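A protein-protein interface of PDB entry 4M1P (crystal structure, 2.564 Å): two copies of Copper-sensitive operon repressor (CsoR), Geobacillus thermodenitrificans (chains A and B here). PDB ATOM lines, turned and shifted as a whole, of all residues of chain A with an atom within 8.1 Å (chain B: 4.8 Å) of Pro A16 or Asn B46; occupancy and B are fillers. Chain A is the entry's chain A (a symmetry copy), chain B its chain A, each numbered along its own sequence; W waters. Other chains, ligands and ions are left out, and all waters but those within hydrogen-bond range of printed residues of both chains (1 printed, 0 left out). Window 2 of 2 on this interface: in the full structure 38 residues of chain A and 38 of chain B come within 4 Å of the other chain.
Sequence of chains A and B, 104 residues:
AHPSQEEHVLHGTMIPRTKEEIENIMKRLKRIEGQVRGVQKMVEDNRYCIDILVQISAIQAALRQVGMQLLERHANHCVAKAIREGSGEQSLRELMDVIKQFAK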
ATOM      1  N   HIS A  11      -7.643   8.428  -2.203  1.00  0.00           N
ATOM      2  CA  HIS A  11      -7.524   8.982  -3.551  1.00  0.00           C
ATOM      3  C   HIS A  11      -6.415   8.295  -4.334  1.00  0.00           C
ATOM      4  O   HIS A  11      -5.697   7.454  -3.792  1.00  0.00           O
ATOM      5  CB  HIS A  11      -7.285  10.496  -3.503  1.00  0.00           C
ATOM      6  CG  HIS A  11      -6.088  10.901  -2.691  1.00  0.00           C
ATOM      7  ND1 HIS A  11      -4.808  10.509  -3.008  1.00  0.00           N
ATOM      8  CD2 HIS A  11      -5.987  11.669  -1.582  1.00  0.00           C
ATOM      9  CE1 HIS A  11      -3.962  11.015  -2.122  1.00  0.00           C
ATOM     10  NE2 HIS A  11      -4.654  11.722  -1.249  1.00  0.00           N
ATOM     11  N   THR A  13      -2.851   7.645  -6.515  1.00  0.00           N
ATOM     12  CA  THR A  13      -1.449   7.789  -6.132  1.00  0.00           C
ATOM     13  C   THR A  13      -0.996   9.244  -6.216  1.00  0.00           C
ATOM     14  O   THR A  13      -1.352   9.954  -7.162  1.00  0.00           O
ATOM     15  CB  THR A  13      -0.538   6.980  -7.066  1.00  0.00           C
ATOM     16  OG1 THR A  13      -1.040   5.645  -7.196  1.00  0.00           O
ATOM     17  CG2 THR A  13       0.880   6.940  -6.528  1.00  0.00           C
ATOM     18  N   MET A  14      -0.210   9.691  -5.237  1.00  0.00           N
ATOM     19  CA  MET A  14       0.382  11.027  -5.303  1.00  0.00           C
ATOM     20  C   MET A  14       1.875  11.025  -4.971  1.00  0.00           C
ATOM     21  O   MET A  14       2.300  10.436  -3.978  1.00  0.00           O
ATOM     22  CB  MET A  14      -0.346  12.000  -4.374  1.00  0.00           C
ATOM     23  CG  MET A  14       0.211  13.413  -4.441  1.00  0.00           C
ATOM     24  SD  MET A  14      -0.465  14.504  -3.187  1.00  0.00           S
ATOM     25  CE  MET A  14       0.346  16.045  -3.618  1.00  0.00           C
ATOM     26  N   ILE A  15       2.668  11.680  -5.813  1.00  0.00           N
ATOM     27  CA  ILE A  15       4.057  11.967  -5.476  1.00  0.00           C
ATOM     28  C   ILE A  15       4.062  13.277  -4.694  1.00  0.00           C
ATOM     29  O   ILE A  15       3.624  14.304  -5.210  1.00  0.00           O
ATOM     30  CB  ILE A  15       4.930  12.154  -6.730  1.00  0.00           C
ATOM     31  CG1 ILE A  15       4.643  11.071  -7.774  1.00  0.00           C
ATOM     32  CG2 ILE A  15       6.409  12.180  -6.344  1.00  0.00           C
ATOM     33  CD1 ILE A  15       5.720  10.021  -7.877  1.00  0.00           C
ATOM     34  N   PRO A  16       4.552  13.246  -3.445  1.00  0.00           N
ATOM     35  CA  PRO A  16       4.519  14.430  -2.573  1.00  0.00           C
ATOM     36  C   PRO A  16       5.362  15.574  -3.132  1.00  0.00           C
ATOM     37  O   PRO A  16       6.358  15.315  -3.804  1.00  0.00           O
ATOM     38  CB  PRO A  16       5.142  13.921  -1.269  1.00  0.00           C
ATOM     39  CG  PRO A  16       5.016  12.430  -1.327  1.00  0.00           C
ATOM     40  CD  PRO A  16       5.154  12.081  -2.775  1.00  0.00           C
ATOM     41  N   ARG A  17       4.972  16.816  -2.858  1.00  0.00           N
ATOM     42  CA  ARG A  17       5.727  17.970  -3.339  1.00  0.00           C
ATOM     43  C   ARG A  17       6.990  18.201  -2.528  1.00  0.00           C
ATOM     44  O   ARG A  17       7.028  17.930  -1.329  1.00  0.00           O
ATOM     45  CB  ARG A  17       4.869  19.232  -3.310  1.00  0.00           C
ATOM     46  CG  ARG A  17       3.667  19.136  -4.200  1.00  0.00           C
ATOM     47  CD  ARG A  17       2.759  20.337  -4.098  1.00  0.00           C
ATOM     48  NE  ARG A  17       1.508  20.017  -4.766  1.00  0.00           N
ATOM     49  CZ  ARG A  17       0.438  19.540  -4.141  1.00  0.00           C
ATOM     50  NH1 ARG A  17       0.455  19.365  -2.825  1.00  0.00           N
ATOM     51  NH2 ARG A  17      -0.657  19.254  -4.831  1.00  0.00           N
ATOM     52  N   THR A  18       8.020  18.709  -3.198  1.00  0.00           N
ATOM     53  CA  THR A  18       9.286  19.048  -2.555  1.00  0.00           C
ATOM     54  C   THR A  18       9.152  20.370  -1.808  1.00  0.00           C
ATOM     55  O   THR A  18       8.119  21.031  -1.901  1.00  0.00           O
ATOM     56  CB  THR A  18      10.402  19.194  -3.601  1.00  0.00           C
ATOM     57  OG1 THR A  18      10.058  20.235  -4.522  1.00  0.00           O
ATOM     58  CG2 THR A  18      10.585  17.894  -4.367  1.00  0.00           C
ATOM     59  N   LYS A  19      10.188  20.754  -1.063  1.00  0.00           N
ATOM     60  CA  LYS A  19      10.235  22.087  -0.475  1.00  0.00           C
ATOM     61  C   LYS A  19      10.246  23.089  -1.620  1.00  0.00           C
ATOM     62  O   LYS A  19       9.644  24.161  -1.544  1.00  0.00           O
ATOM     63  CB  LYS A  19      11.485  22.255   0.386  1.00  0.00           C
ATOM     64  N   GLU A  21       9.023  22.698  -4.945  1.00  0.00           N
ATOM     65  CA  GLU A  21       7.736  22.795  -5.633  1.00  0.00           C
ATOM     66  C   GLU A  21       6.739  23.654  -4.867  1.00  0.00           C
ATOM     67  O   GLU A  21       6.074  24.513  -5.448  1.00  0.00           O
ATOM     68  CB  GLU A  21       7.130  21.408  -5.847  1.00  0.00           C
ATOM     69  CG  GLU A  21       7.771  20.584  -6.945  1.00  0.00           C
ATOM     70  CD  GLU A  21       7.001  19.307  -7.218  1.00  0.00           C
ATOM     71  OE1 GLU A  21       6.334  19.225  -8.274  1.00  0.00           O
ATOM     72  OE2 GLU A  21       7.058  18.389  -6.374  1.00  0.00           O
ATOM     73  N   ILE A  22       6.631  23.405  -3.566  1.00  0.00           N
ATOM     74  CA  ILE A  22       5.728  24.166  -2.716  1.00  0.00           C
ATOM     75  C   ILE A  22       6.092  25.649  -2.738  1.00  0.00           C
ATOM     76  O   ILE A  22       5.221  26.503  -2.907  1.00  0.00           O
ATOM     77  CB  ILE A  22       5.725  23.635  -1.270  1.00  0.00           C
ATOM     78  CG1 ILE A  22       5.113  22.233  -1.217  1.00  0.00           C
ATOM     79  CG2 ILE A  22       4.958  24.572  -0.354  1.00  0.00           C
ATOM     80  CD1 ILE A  22       5.081  21.626   0.177  1.00  0.00           C
ATOM     81  N   ARG A  73       2.116  18.511 -13.909  1.00  0.00           N
ATOM     82  CA  ARG A  73       2.862  17.876 -12.838  1.00  0.00           C
ATOM     83  C   ARG A  73       2.143  16.603 -12.409  1.00  0.00           C
ATOM     84  O   ARG A  73       2.753  15.535 -12.343  1.00  0.00           O
ATOM     85  CB  ARG A  73       3.033  18.834 -11.657  1.00  0.00           C
ATOM     86  CG  ARG A  73       4.167  18.486 -10.712  1.00  0.00           C
ATOM     87  CD  ARG A  73       3.766  17.405  -9.718  1.00  0.00           C
ATOM     88  NE  ARG A  73       4.657  17.372  -8.564  1.00  0.00           N
ATOM     89  CZ  ARG A  73       4.493  16.569  -7.521  1.00  0.00           C
ATOM     90  NH1 ARG A  73       3.471  15.721  -7.492  1.00  0.00           N
ATOM     91  NH2 ARG A  73       5.349  16.611  -6.509  1.00  0.00           N
ATOM     92  N   HIS A  77       3.842  12.856 -13.222  1.00  0.00           N
ATOM     93  CA  HIS A  77       4.408  12.147 -12.082  1.00  0.00           C
ATOM     94  C   HIS A  77       3.415  11.239 -11.375  1.00  0.00           C
ATOM     95  O   HIS A  77       3.563  10.015 -11.396  1.00  0.00           O
ATOM     96  CB  HIS A  77       5.010  13.143 -11.098  1.00  0.00           C
ATOM     97  CG  HIS A  77       6.145  13.933 -11.677  1.00  0.00           C
ATOM     98  ND1 HIS A  77       6.169  15.307 -11.674  1.00  0.00           N
ATOM     99  CD2 HIS A  77       7.279  13.531 -12.295  1.00  0.00           C
ATOM    100  CE1 HIS A  77       7.281  15.725 -12.262  1.00  0.00           C
ATOM    101  NE2 HIS A  77       7.970  14.665 -12.645  1.00  0.00           N
ATOM    102  N   CYS A  78       2.404  11.834 -10.753  1.00  0.00           N
ATOM    103  CA  CYS A  78       1.442  11.071  -9.957  1.00  0.00           C
ATOM    104  C   CYS A  78       0.654  10.040 -10.779  1.00  0.00           C
ATOM    105  O   CYS A  78       0.642   8.855 -10.444  1.00  0.00           O
ATOM    106  CB  CYS A  78       0.484  12.008  -9.212  1.00  0.00           C
ATOM    107  SG  CYS A  78       1.287  13.211  -8.114  1.00  0.00           S
ATOM    108  N   LYS A  81       2.912   7.397 -12.147  1.00  0.00           N
ATOM    109  CA  LYS A  81       3.265   6.418 -11.124  1.00  0.00           C
ATOM    110  C   LYS A  81       2.155   5.378 -10.956  1.00  0.00           C
ATOM    111  O   LYS A  81       2.422   4.176 -10.881  1.00  0.00           O
ATOM    112  CB  LYS A  81       3.574   7.100  -9.785  1.00  0.00           C
ATOM    113  CG  LYS A  81       3.938   6.125  -8.672  1.00  0.00           C
ATOM    114  CD  LYS A  81       4.418   6.834  -7.414  1.00  0.00           C
ATOM    115  N   MET B  42      -3.825  24.413   1.098  1.00  0.00           N
ATOM    116  CA  MET B  42      -3.868  23.089   0.478  1.00  0.00           C
ATOM    117  C   MET B  42      -2.497  22.656  -0.033  1.00  0.00           C
ATOM    118  O   MET B  42      -2.070  21.525   0.204  1.00  0.00           O
ATOM    119  CB  MET B  42      -4.882  23.055  -0.668  1.00  0.00           C
ATOM    120  CG  MET B  42      -6.327  23.190  -0.219  1.00  0.00           C
ATOM    121  SD  MET B  42      -7.507  23.038  -1.572  1.00  0.00           S
ATOM    122  CE  MET B  42      -7.356  21.289  -1.915  1.00  0.00           C
ATOM    123  N   VAL B  43      -1.810  23.558  -0.730  1.00  0.00           N
ATOM    124  CA  VAL B  43      -0.488  23.266  -1.274  1.00  0.00           C
ATOM    125  C   VAL B  43       0.506  23.007  -0.145  1.00  0.00           C
ATOM    126  O   VAL B  43       1.319  22.080  -0.218  1.00  0.00           O
ATOM    127  CB  VAL B  43       0.028  24.417  -2.157  1.00  0.00           C
ATOM    128  CG1 VAL B  43       1.440  24.137  -2.643  1.00  0.00           C
ATOM    129  CG2 VAL B  43      -0.903  24.637  -3.342  1.00  0.00           C
ATOM    130  N   GLU B  44       0.430  23.831   0.898  1.00  0.00           N
ATOM    131  CA  GLU B  44       1.305  23.692   2.060  1.00  0.00           C
ATOM    132  C   GLU B  44       1.068  22.366   2.778  1.00  0.00           C
ATOM    133  O   GLU B  44       2.013  21.684   3.181  1.00  0.00           O
ATOM    134  CB  GLU B  44       1.098  24.854   3.038  1.00  0.00           C
ATOM    135  CG  GLU B  44       1.658  26.197   2.565  1.00  0.00           C
ATOM    136  CD  GLU B  44       1.399  27.327   3.552  1.00  0.00           C
ATOM    137  OE1 GLU B  44       0.543  27.165   4.448  1.00  0.00           O
ATOM    138  OE2 GLU B  44       2.055  28.382   3.434  1.00  0.00           O
ATOM    139  N   ASP B  45      -0.200  21.999   2.929  1.00  0.00           N
ATOM    140  CA  ASP B  45      -0.558  20.766   3.614  1.00  0.00           C
ATOM    141  C   ASP B  45      -0.301  19.560   2.721  1.00  0.00           C
ATOM    142  O   ASP B  45      -0.624  18.430   3.083  1.00  0.00           O
ATOM    143  CB  ASP B  45      -2.019  20.819   4.061  1.00  0.00           C
ATOM    144  CG  ASP B  45      -2.280  21.941   5.048  1.00  0.00           C
ATOM    145  OD1 ASP B  45      -1.442  22.864   5.125  1.00  0.00           O
ATOM    146  OD2 ASP B  45      -3.318  21.906   5.742  1.00  0.00           O
ATOM    147  N   ASN B  46       0.291  19.816   1.557  1.00  0.00           N
ATOM    148  CA  ASN B  46       0.579  18.779   0.570  1.00  0.00           C
ATOM    149  C   ASN B  46      -0.665  17.966   0.183  1.00  0.00           C
ATOM    150  O   ASN B  46      -0.607  16.744   0.066  1.00  0.00           O
ATOM    151  CB  ASN B  46       1.700  17.856   1.068  1.00  0.00           C
ATOM    152  CG  ASN B  46       2.794  17.648   0.031  1.00  0.00           C
ATOM    153  OD1 ASN B  46       2.525  17.565  -1.167  1.00  0.00           O
ATOM    154  ND2 ASN B  46       4.038  17.557   0.493  1.00  0.00           N
ATOM    155  N   ARG B  47      -1.787  18.653  -0.012  1.00  0.00           N
ATOM    156  CA  ARG B  47      -3.029  17.983  -0.378  1.00  0.00           C
ATOM    157  C   ARG B  47      -2.997  17.495  -1.824  1.00  0.00           C
ATOM    158  O   ARG B  47      -2.144  17.917  -2.610  1.00  0.00           O
ATOM    159  CB  ARG B  47      -4.243  18.881  -0.104  1.00  0.00           C
ATOM    160  CG  ARG B  47      -4.602  18.960   1.387  1.00  0.00           C
ATOM    161  CD  ARG B  47      -6.035  19.423   1.632  1.00  0.00           C
ATOM    162  NE  ARG B  47      -7.021  18.510   1.057  1.00  0.00           N
ATOM    163  CZ  ARG B  47      -8.321  18.776   0.962  1.00  0.00           C
ATOM    164  NH1 ARG B  47      -8.802  19.928   1.407  1.00  0.00           N
ATOM    165  NH2 ARG B  47      -9.145  17.891   0.418  1.00  0.00           N
ATOM    166  N   TYR B  48      -3.914  16.587  -2.150  1.00  0.00           N
ATOM    167  CA  TYR B  48      -3.967  15.944  -3.461  1.00  0.00           C
ATOM    168  C   TYR B  48      -4.130  16.955  -4.588  1.00  0.00           C
ATOM    169  O   TYR B  48      -4.979  17.849  -4.505  1.00  0.00           O
ATOM    170  CB  TYR B  48      -5.122  14.944  -3.496  1.00  0.00           C
ATOM    171  CG  TYR B  48      -5.087  13.956  -4.648  1.00  0.00           C
ATOM    172  CD1 TYR B  48      -6.250  13.618  -5.333  1.00  0.00           C
ATOM    173  CD2 TYR B  48      -3.898  13.352  -5.041  1.00  0.00           C
ATOM    174  CE1 TYR B  48      -6.233  12.710  -6.366  1.00  0.00           C
ATOM    175  CE2 TYR B  48      -3.872  12.445  -6.080  1.00  0.00           C
ATOM    176  CZ  TYR B  48      -5.043  12.129  -6.739  1.00  0.00           C
ATOM    177  OH  TYR B  48      -5.016  11.224  -7.775  1.00  0.00           O
HETATM  178  O   HOH W   1      -3.004   9.582  -9.378  1.00  0.00           O
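N of Arg A17 is in hydrogen-bond range of OD1 of Asn B46 (3.1 Å).
The backbone carbonyl oxygen (O) of Arg B47 lies within hydrogen-bond range of the guanidinium group (NH1) of Arg A17, at 3.0 Å.
The backbone carbonyl oxygen (O) of Met B42 lies within hydrogen-bond range of the backbone NH (N) of Arg B47, 2.9 Å away.
O of Pro A16 sits at hydrogen-bond distance from NH2 of Arg A73 (3.2 Å).
Among the printed residues, merely in contact across the chains: His A11 with Tyr B48 (3.6 Å), Thr A13 with Tyr B48 (3.7 Å), Met A14 with Asn B46 (3.6 Å), Met A14 with Arg B47 (3.3 Å), Met A14 with Tyr B48 (3.8 Å), Pro A16 with Asn B46 (3.97 Å), Arg A17 with Val B43 (3.9 Å) and Ile A22 with Val B43 (3.8 Å).
Printed residues of chain B within 4 Å of Thr A13: Tyr B48 (3.7 Å).
Of chain B, only Asn B46 comes within 4 Å of Pro A16.
Of the printed residues of chain A, Asn B46 touches Met A14 (3.6 Å), Pro A16 (3.97 Å) and Arg A17 (3.1 Å).
Of the printed residues of chain A, Tyr B48 touches His A11, Thr A13 and Met A14.
The nearest printed residue of chain B that does not touch Ile A22 is Asn B46 (4.2 Å).
Hydrophobic or aromatic side chains of chain A within 4 Å of the printed part of chain B: His A11, Met A14 and Ile A22.
Of the 7 printed residues of chain B, 4 touch a printed residue of chain A.
Hydrophobic or aromatic side chains of chain B within 4 Å of the printed part of chain A: Tyr B48.
No position is printed for both chains.
Of the 10 pairs that touch across the chains among the printed residues, none has its exchanged pair printed and touching as well.
Water W1 lies within hydrogen-bond range of O of Thr A13 (2.8 Å) and OH of Tyr B48 (3.1 Å).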
